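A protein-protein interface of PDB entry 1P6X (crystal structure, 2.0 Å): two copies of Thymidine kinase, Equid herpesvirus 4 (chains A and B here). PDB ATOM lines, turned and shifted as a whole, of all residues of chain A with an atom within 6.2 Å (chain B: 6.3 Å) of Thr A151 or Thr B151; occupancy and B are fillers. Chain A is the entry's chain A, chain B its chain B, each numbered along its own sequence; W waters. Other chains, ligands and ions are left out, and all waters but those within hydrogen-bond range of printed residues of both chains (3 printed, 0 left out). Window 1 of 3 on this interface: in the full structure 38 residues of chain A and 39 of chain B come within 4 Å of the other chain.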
ATOM      1  N   THR A  88       9.730   5.229 -18.603  1.00  0.00           N
ATOM      2  CA  THR A  88       9.725   4.665 -19.964  1.00  0.00           C
ATOM      3  C   THR A  88       9.791   5.736 -21.049  1.00  0.00           C
ATOM      4  O   THR A  88      10.285   5.498 -22.137  1.00  0.00           O
ATOM      5  CB  THR A  88       8.470   3.820 -20.221  1.00  0.00           C
ATOM      6  OG1 THR A  88       7.327   4.672 -20.151  1.00  0.00           O
ATOM      7  CG2 THR A  88       8.239   2.818 -19.103  1.00  0.00           C
ATOM      8  N   LEU A  92      10.995   5.375 -24.956  1.00  0.00           N
ATOM      9  CA  LEU A  92      10.052   5.301 -26.072  1.00  0.00           C
ATOM     10  C   LEU A  92      10.367   6.335 -27.135  1.00  0.00           C
ATOM     11  O   LEU A  92      10.281   6.033 -28.339  1.00  0.00           O
ATOM     12  CB  LEU A  92       8.592   5.427 -25.629  1.00  0.00           C
ATOM     13  CG  LEU A  92       8.055   4.422 -24.617  1.00  0.00           C
ATOM     14  CD1 LEU A  92       6.590   4.713 -24.293  1.00  0.00           C
ATOM     15  CD2 LEU A  92       8.165   2.976 -25.162  1.00  0.00           C
ATOM     16  N   THR A 127       9.349  -0.927 -19.253  1.00  0.00           N
ATOM     17  CA  THR A 127       7.953  -1.276 -19.506  1.00  0.00           C
ATOM     18  C   THR A 127       7.592  -2.635 -18.946  1.00  0.00           C
ATOM     19  O   THR A 127       6.421  -2.903 -18.727  1.00  0.00           O
ATOM     20  CB  THR A 127       7.609  -1.244 -21.015  1.00  0.00           C
ATOM     21  OG1 THR A 127       8.538  -2.079 -21.707  1.00  0.00           O
ATOM     22  CG2 THR A 127       7.834   0.168 -21.601  1.00  0.00           C
ATOM     23  N   MET A 146      -0.010  -4.501 -16.421  1.00  0.00           N
ATOM     24  CA  MET A 146      -0.543  -4.655 -17.765  1.00  0.00           C
ATOM     25  C   MET A 146      -0.458  -3.343 -18.520  1.00  0.00           C
ATOM     26  O   MET A 146      -0.125  -3.348 -19.700  1.00  0.00           O
ATOM     27  CB  MET A 146      -1.987  -5.166 -17.747  1.00  0.00           C
ATOM     28  CG  MET A 146      -2.079  -6.657 -17.470  1.00  0.00           C
ATOM     29  SD  MET A 146      -1.592  -7.530 -18.972  1.00  0.00           S
ATOM     30  CE  MET A 146      -1.930  -9.150 -18.531  1.00  0.00           C
ATOM     31  N   ALA A 147      -0.730  -2.231 -17.832  1.00  0.00           N
ATOM     32  CA  ALA A 147      -0.651  -0.914 -18.446  1.00  0.00           C
ATOM     33  C   ALA A 147       0.739  -0.564 -18.926  1.00  0.00           C
ATOM     34  O   ALA A 147       0.885   0.052 -19.992  1.00  0.00           O
ATOM     35  CB  ALA A 147      -1.166   0.176 -17.505  1.00  0.00           C
ATOM     36  N   MET A 148       1.770  -0.909 -18.142  1.00  0.00           N
ATOM     37  CA  MET A 148       3.139  -0.649 -18.610  1.00  0.00           C
ATOM     38  C   MET A 148       3.542  -1.627 -19.715  1.00  0.00           C
ATOM     39  O   MET A 148       4.155  -1.230 -20.686  1.00  0.00           O
ATOM     40  CB  MET A 148       4.159  -0.741 -17.481  1.00  0.00           C
ATOM     41  CG  MET A 148       3.578  -0.708 -16.130  1.00  0.00           C
ATOM     42  SD  MET A 148       4.326   0.676 -15.395  1.00  0.00           S
ATOM     43  CE  MET A 148       3.954   1.745 -16.706  1.00  0.00           C
ATOM     44  N   VAL A 149       3.187  -2.892 -19.546  1.00  0.00           N
ATOM     45  CA  VAL A 149       3.591  -3.940 -20.493  1.00  0.00           C
ATOM     46  C   VAL A 149       3.040  -3.686 -21.913  1.00  0.00           C
ATOM     47  O   VAL A 149       3.749  -3.898 -22.944  1.00  0.00           O
ATOM     48  CB  VAL A 149       3.193  -5.336 -19.985  1.00  0.00           C
ATOM     49  CG1 VAL A 149       3.264  -6.409 -21.115  1.00  0.00           C
ATOM     50  CG2 VAL A 149       4.052  -5.747 -18.829  1.00  0.00           C
ATOM     51  N   ALA A 150       1.776  -3.257 -21.965  1.00  0.00           N
ATOM     52  CA  ALA A 150       1.136  -2.838 -23.215  1.00  0.00           C
ATOM     53  C   ALA A 150       1.912  -1.753 -23.986  1.00  0.00           C
ATOM     54  O   ALA A 150       1.792  -1.655 -25.191  1.00  0.00           O
ATOM     55  CB  ALA A 150      -0.285  -2.346 -22.925  1.00  0.00           C
ATOM     56  N   THR A 151       2.687  -0.925 -23.289  1.00  0.00           N
ATOM     57  CA  THR A 151       3.419   0.149 -23.942  1.00  0.00           C
ATOM     58  C   THR A 151       4.804  -0.277 -24.466  1.00  0.00           C
ATOM     59  O   THR A 151       5.508   0.540 -25.089  1.00  0.00           O
ATOM     60  CB  THR A 151       3.563   1.431 -23.036  1.00  0.00           C
ATOM     61  OG1 THR A 151       4.484   1.178 -21.956  1.00  0.00           O
ATOM     62  CG2 THR A 151       2.241   1.762 -22.302  1.00  0.00           C
ATOM     63  N   LEU A 152       5.210  -1.519 -24.211  1.00  0.00           N
ATOM     64  CA  LEU A 152       6.443  -2.027 -24.831  1.00  0.00           C
ATOM     65  C   LEU A 152       6.372  -1.871 -26.372  1.00  0.00           C
ATOM     66  O   LEU A 152       5.434  -2.355 -27.004  1.00  0.00           O
ATOM     67  CB  LEU A 152       6.649  -3.507 -24.450  1.00  0.00           C
ATOM     68  CG  LEU A 152       7.784  -4.271 -25.184  1.00  0.00           C
ATOM     69  CD1 LEU A 152       9.178  -3.813 -24.704  1.00  0.00           C
ATOM     70  CD2 LEU A 152       7.605  -5.753 -24.949  1.00  0.00           C
ATOM     71  N   PRO A 153       7.334  -1.200 -26.996  1.00  0.00           N
ATOM     72  CA  PRO A 153       7.289  -1.056 -28.450  1.00  0.00           C
ATOM     73  C   PRO A 153       7.820  -2.327 -29.100  1.00  0.00           C
ATOM     74  O   PRO A 153       8.682  -2.987 -28.536  1.00  0.00           O
ATOM     75  CB  PRO A 153       8.240   0.104 -28.723  1.00  0.00           C
ATOM     76  CG  PRO A 153       9.208   0.070 -27.609  1.00  0.00           C
ATOM     77  CD  PRO A 153       8.492  -0.508 -26.403  1.00  0.00           C
ATOM     78  N   LYS A 279       6.636  -8.870 -29.571  1.00  0.00           N
ATOM     79  CA  LYS A 279       7.485  -7.688 -29.455  1.00  0.00           C
ATOM     80  C   LYS A 279       8.927  -8.057 -29.127  1.00  0.00           C
ATOM     81  O   LYS A 279       9.861  -7.292 -29.428  1.00  0.00           O
ATOM     82  CB  LYS A 279       6.923  -6.715 -28.425  1.00  0.00           C
ATOM     83  CG  LYS A 279       5.748  -5.940 -28.956  1.00  0.00           C
ATOM     84  CD  LYS A 279       4.990  -5.260 -27.825  1.00  0.00           C
ATOM     85  CE  LYS A 279       3.663  -4.671 -28.340  1.00  0.00           C
ATOM     86  NZ  LYS A 279       3.092  -3.735 -27.321  1.00  0.00           N
ATOM     87  N   THR B  88      -5.713   3.860 -21.625  1.00  0.00           N
ATOM     88  CA  THR B  88      -5.080   3.492 -22.894  1.00  0.00           C
ATOM     89  C   THR B  88      -4.915   1.996 -23.063  1.00  0.00           C
ATOM     90  O   THR B  88      -4.917   1.513 -24.185  1.00  0.00           O
ATOM     91  CB  THR B  88      -3.716   4.165 -23.085  1.00  0.00           C
ATOM     92  OG1 THR B  88      -2.758   3.555 -22.203  1.00  0.00           O
ATOM     93  CG2 THR B  88      -3.753   5.626 -22.654  1.00  0.00           C
ATOM     94  N   LEU B  92      -4.470  -0.196 -26.638  1.00  0.00           N
ATOM     95  CA  LEU B  92      -3.150  -0.611 -27.066  1.00  0.00           C
ATOM     96  C   LEU B  92      -3.193  -2.100 -27.357  1.00  0.00           C
ATOM     97  O   LEU B  92      -2.631  -2.551 -28.334  1.00  0.00           O
ATOM     98  CB  LEU B  92      -2.114  -0.304 -25.978  1.00  0.00           C
ATOM     99  CG  LEU B  92      -1.782   1.165 -25.762  1.00  0.00           C
ATOM    100  CD1 LEU B  92      -0.570   1.320 -24.888  1.00  0.00           C
ATOM    101  CD2 LEU B  92      -1.533   1.912 -27.088  1.00  0.00           C
ATOM    102  N   ASP B  96      -2.664  -3.648 -30.974  1.00  0.00           N
ATOM    103  CA  ASP B  96      -1.638  -4.681 -31.198  1.00  0.00           C
ATOM    104  C   ASP B  96      -2.260  -5.956 -31.829  1.00  0.00           C
ATOM    105  O   ASP B  96      -1.676  -6.566 -32.722  1.00  0.00           O
ATOM    106  CB  ASP B  96      -0.946  -5.044 -29.896  1.00  0.00           C
ATOM    107  CG  ASP B  96       0.210  -4.112 -29.536  1.00  0.00           C
ATOM    108  OD1 ASP B  96       0.817  -3.467 -30.431  1.00  0.00           O
ATOM    109  OD2 ASP B  96       0.599  -4.004 -28.344  1.00  0.00           O
ATOM    110  N   PRO B 123      -6.752   4.703 -30.592  1.00  0.00           N
ATOM    111  CA  PRO B 123      -5.824   4.933 -29.478  1.00  0.00           C
ATOM    112  C   PRO B 123      -5.437   6.420 -29.244  1.00  0.00           C
ATOM    113  O   PRO B 123      -5.072   6.745 -28.150  1.00  0.00           O
ATOM    114  CB  PRO B 123      -4.604   4.099 -29.868  1.00  0.00           C
ATOM    115  CG  PRO B 123      -5.207   2.932 -30.643  1.00  0.00           C
ATOM    116  CD  PRO B 123      -6.331   3.546 -31.433  1.00  0.00           C
ATOM    117  N   THR B 127      -4.387   8.305 -25.556  1.00  0.00           N
ATOM    118  CA  THR B 127      -2.966   8.622 -25.438  1.00  0.00           C
ATOM    119  C   THR B 127      -2.645  10.090 -25.671  1.00  0.00           C
ATOM    120  O   THR B 127      -1.603  10.561 -25.213  1.00  0.00           O
ATOM    121  CB  THR B 127      -2.032   7.731 -26.376  1.00  0.00           C
ATOM    122  OG1 THR B 127      -2.392   7.928 -27.750  1.00  0.00           O
ATOM    123  CG2 THR B 127      -2.270   6.235 -26.132  1.00  0.00           C
ATOM    124  N   MET B 146       3.489  14.110 -22.020  1.00  0.00           N
ATOM    125  CA  MET B 146       4.556  13.485 -22.812  1.00  0.00           C
ATOM    126  C   MET B 146       4.611  11.984 -22.614  1.00  0.00           C
ATOM    127  O   MET B 146       4.839  11.233 -23.585  1.00  0.00           O
ATOM    128  CB  MET B 146       5.935  14.087 -22.477  1.00  0.00           C
ATOM    129  CG  MET B 146       6.235  15.413 -23.147  1.00  0.00           C
ATOM    130  SD  MET B 146       6.292  15.269 -24.945  1.00  0.00           S
ATOM    131  CE  MET B 146       6.923  16.793 -25.391  1.00  0.00           C
ATOM    132  N   ALA B 147       4.389  11.533 -21.385  1.00  0.00           N
ATOM    133  CA  ALA B 147       4.408  10.097 -21.109  1.00  0.00           C
ATOM    134  C   ALA B 147       3.277   9.361 -21.825  1.00  0.00           C
ATOM    135  O   ALA B 147       3.481   8.237 -22.306  1.00  0.00           O
ATOM    136  CB  ALA B 147       4.351   9.799 -19.605  1.00  0.00           C
ATOM    137  N   MET B 148       2.080   9.955 -21.849  1.00  0.00           N
ATOM    138  CA  MET B 148       0.949   9.349 -22.572  1.00  0.00           C
ATOM    139  C   MET B 148       1.165   9.437 -24.082  1.00  0.00           C
ATOM    140  O   MET B 148       0.931   8.463 -24.800  1.00  0.00           O
ATOM    141  CB  MET B 148      -0.422   9.992 -22.258  1.00  0.00           C
ATOM    142  CG  MET B 148      -0.724  10.331 -20.817  1.00  0.00           C
ATOM    143  SD  MET B 148      -0.981   8.894 -19.915  1.00  0.00           S
ATOM    144  CE  MET B 148      -2.184   8.000 -20.992  1.00  0.00           C
ATOM    145  N   VAL B 149       1.615  10.599 -24.549  1.00  0.00           N
ATOM    146  CA  VAL B 149       1.763  10.835 -25.993  1.00  0.00           C
ATOM    147  C   VAL B 149       2.779   9.865 -26.635  1.00  0.00           C
ATOM    148  O   VAL B 149       2.532   9.367 -27.729  1.00  0.00           O
ATOM    149  CB  VAL B 149       2.126  12.291 -26.298  1.00  0.00           C
ATOM    150  CG1 VAL B 149       2.474  12.487 -27.766  1.00  0.00           C
ATOM    151  CG2 VAL B 149       0.923  13.258 -25.901  1.00  0.00           C
ATOM    152  N   ALA B 150       3.879   9.588 -25.926  1.00  0.00           N
ATOM    153  CA  ALA B 150       4.905   8.672 -26.415  1.00  0.00           C
ATOM    154  C   ALA B 150       4.385   7.240 -26.594  1.00  0.00           C
ATOM    155  O   ALA B 150       5.006   6.467 -27.317  1.00  0.00           O
ATOM    156  CB  ALA B 150       6.139   8.684 -25.502  1.00  0.00           C
ATOM    157  N   THR B 151       3.285   6.882 -25.934  1.00  0.00           N
ATOM    158  CA  THR B 151       2.674   5.550 -26.090  1.00  0.00           C
ATOM    159  C   THR B 151       1.676   5.418 -27.236  1.00  0.00           C
ATOM    160  O   THR B 151       1.133   4.340 -27.472  1.00  0.00           O
ATOM    161  CB  THR B 151       2.006   5.030 -24.768  1.00  0.00           C
ATOM    162  OG1 THR B 151       0.793   5.758 -24.512  1.00  0.00           O
ATOM    163  CG2 THR B 151       2.867   5.281 -23.569  1.00  0.00           C
ATOM    164  N   LEU B 152       1.412   6.510 -27.944  1.00  0.00           N
ATOM    165  CA  LEU B 152       0.597   6.400 -29.147  1.00  0.00           C
ATOM    166  C   LEU B 152       1.285   5.362 -30.071  1.00  0.00           C
ATOM    167  O   LEU B 152       2.484   5.474 -30.314  1.00  0.00           O
ATOM    168  CB  LEU B 152       0.495   7.764 -29.847  1.00  0.00           C
ATOM    169  CG  LEU B 152      -0.314   7.873 -31.164  1.00  0.00           C
ATOM    170  CD1 LEU B 152      -1.827   7.791 -30.950  1.00  0.00           C
ATOM    171  CD2 LEU B 152       0.059   9.142 -31.896  1.00  0.00           C
ATOM    172  N   PRO B 153       0.552   4.347 -30.548  1.00  0.00           N
ATOM    173  CA  PRO B 153       1.082   3.424 -31.578  1.00  0.00           C
ATOM    174  C   PRO B 153       1.029   4.026 -32.991  1.00  0.00           C
ATOM    175  O   PRO B 153       0.163   4.844 -33.283  1.00  0.00           O
ATOM    176  CB  PRO B 153       0.146   2.209 -31.496  1.00  0.00           C
ATOM    177  CG  PRO B 153      -1.173   2.764 -30.907  1.00  0.00           C
ATOM    178  CD  PRO B 153      -0.823   3.998 -30.136  1.00  0.00           C
ATOM    179  N   LYS B 279       3.154   9.132 -36.568  1.00  0.00           N
ATOM    180  CA  LYS B 279       2.140   8.148 -36.167  1.00  0.00           C
ATOM    181  C   LYS B 279       0.748   8.472 -36.703  1.00  0.00           C
ATOM    182  O   LYS B 279      -0.065   7.570 -36.899  1.00  0.00           O
ATOM    183  CB  LYS B 279       2.114   7.971 -34.650  1.00  0.00           C
ATOM    184  CG  LYS B 279       3.376   7.274 -34.130  1.00  0.00           C
ATOM    185  CD  LYS B 279       3.542   7.503 -32.641  1.00  0.00           C
ATOM    186  CE  LYS B 279       4.789   6.776 -32.153  1.00  0.00           C
ATOM    187  NZ  LYS B 279       4.858   6.939 -30.673  1.00  0.00           N
HETATM  188  O   HOH W   1       5.782   7.154 -21.658  1.00  0.00           O
HETATM  189  O   HOH W   2       2.733  -1.584 -29.773  1.00  0.00           O
HETATM  190  O   HOH W   3      -1.400   0.902 -21.154  1.00  0.00           O
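The side-chain carboxylate (OD2) of Asp B96 is in salt-bridge range of the side-chain amino group (NZ) of Lys A279 (2.7 Å).
The backbone carbonyl oxygen (O) of Met A148 lies within hydrogen-bond range of the side-chain hydroxyl (OG1) of Thr A151, at 2.7 Å.
O of Ala A150 sits at hydrogen-bond distance from NZ of Lys A279 (3.2 Å).
The side-chain amino group of Lys A279 is in hydrogen-bond range of the backbone carbonyl oxygen of Leu A152.
The side-chain hydroxyl of Thr B151 sits at hydrogen-bond distance from the backbone carbonyl oxygen of Met B148, 2.7 Å away.
The side-chain amino group (NZ) of Lys B279 lies within hydrogen-bond range of the backbone carbonyl oxygen (O) of Ala B150, 3.4 Å away.
Of the printed residues of chain B, Ala A150 touches Leu B92.
Thr A151 touches just these residues of chain B: Leu B92 (3.8 Å) and Thr B151 (3.8 Å).
Of the printed residues of chain B, Lys A279 touches Asp B96 (2.7 Å).
Printed residues of chain A within 4 Å of Asp B96: Lys A279 (2.7 Å).
Printed residues of chain A within 4 Å of Ala B150: Leu A92.
Of chain A, only Leu A92 and Thr A151 come within 4 Å of Thr B151.
The nearest residue of chain B that does not touch Thr A151 is Thr B88 (5.3 Å).
The nearest printed residue of chain B that does not touch Leu A92 is Ala B147 (5.1 Å).
Water W1 lies within hydrogen-bond range of O of Ala B147 (2.6 Å) and OG1 of Thr A88 (3.3 Å).
Water W3 lies within hydrogen-bond range of the backbone carbonyl oxygen of Ala A147 and the side-chain hydroxyl of Thr B88.
Water W2 lies within hydrogen-bond range of OD1 of Asp B96 (2.8 Å) and NZ of Lys A279 (3.3 Å).
Leu A92 touches Ala B150, and with the chains exchanged Ala A150 touches Leu B92.
Leu A92 touches Thr B151, and with the chains exchanged Thr A151 touches Leu B92.
Thr B151 touches its own counterpart, Thr A151.
Among the printed residues, pairs that only touch across the chains: Thr A151 with Thr B151, Ala A150 with Leu B92, Leu A92 with Thr B151, Leu A92 with Ala B150 and Thr A151 with Leu B92.
Hydrophobic or aromatic side chains of chain A within 4 Å of the printed part of chain B: Leu A92.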
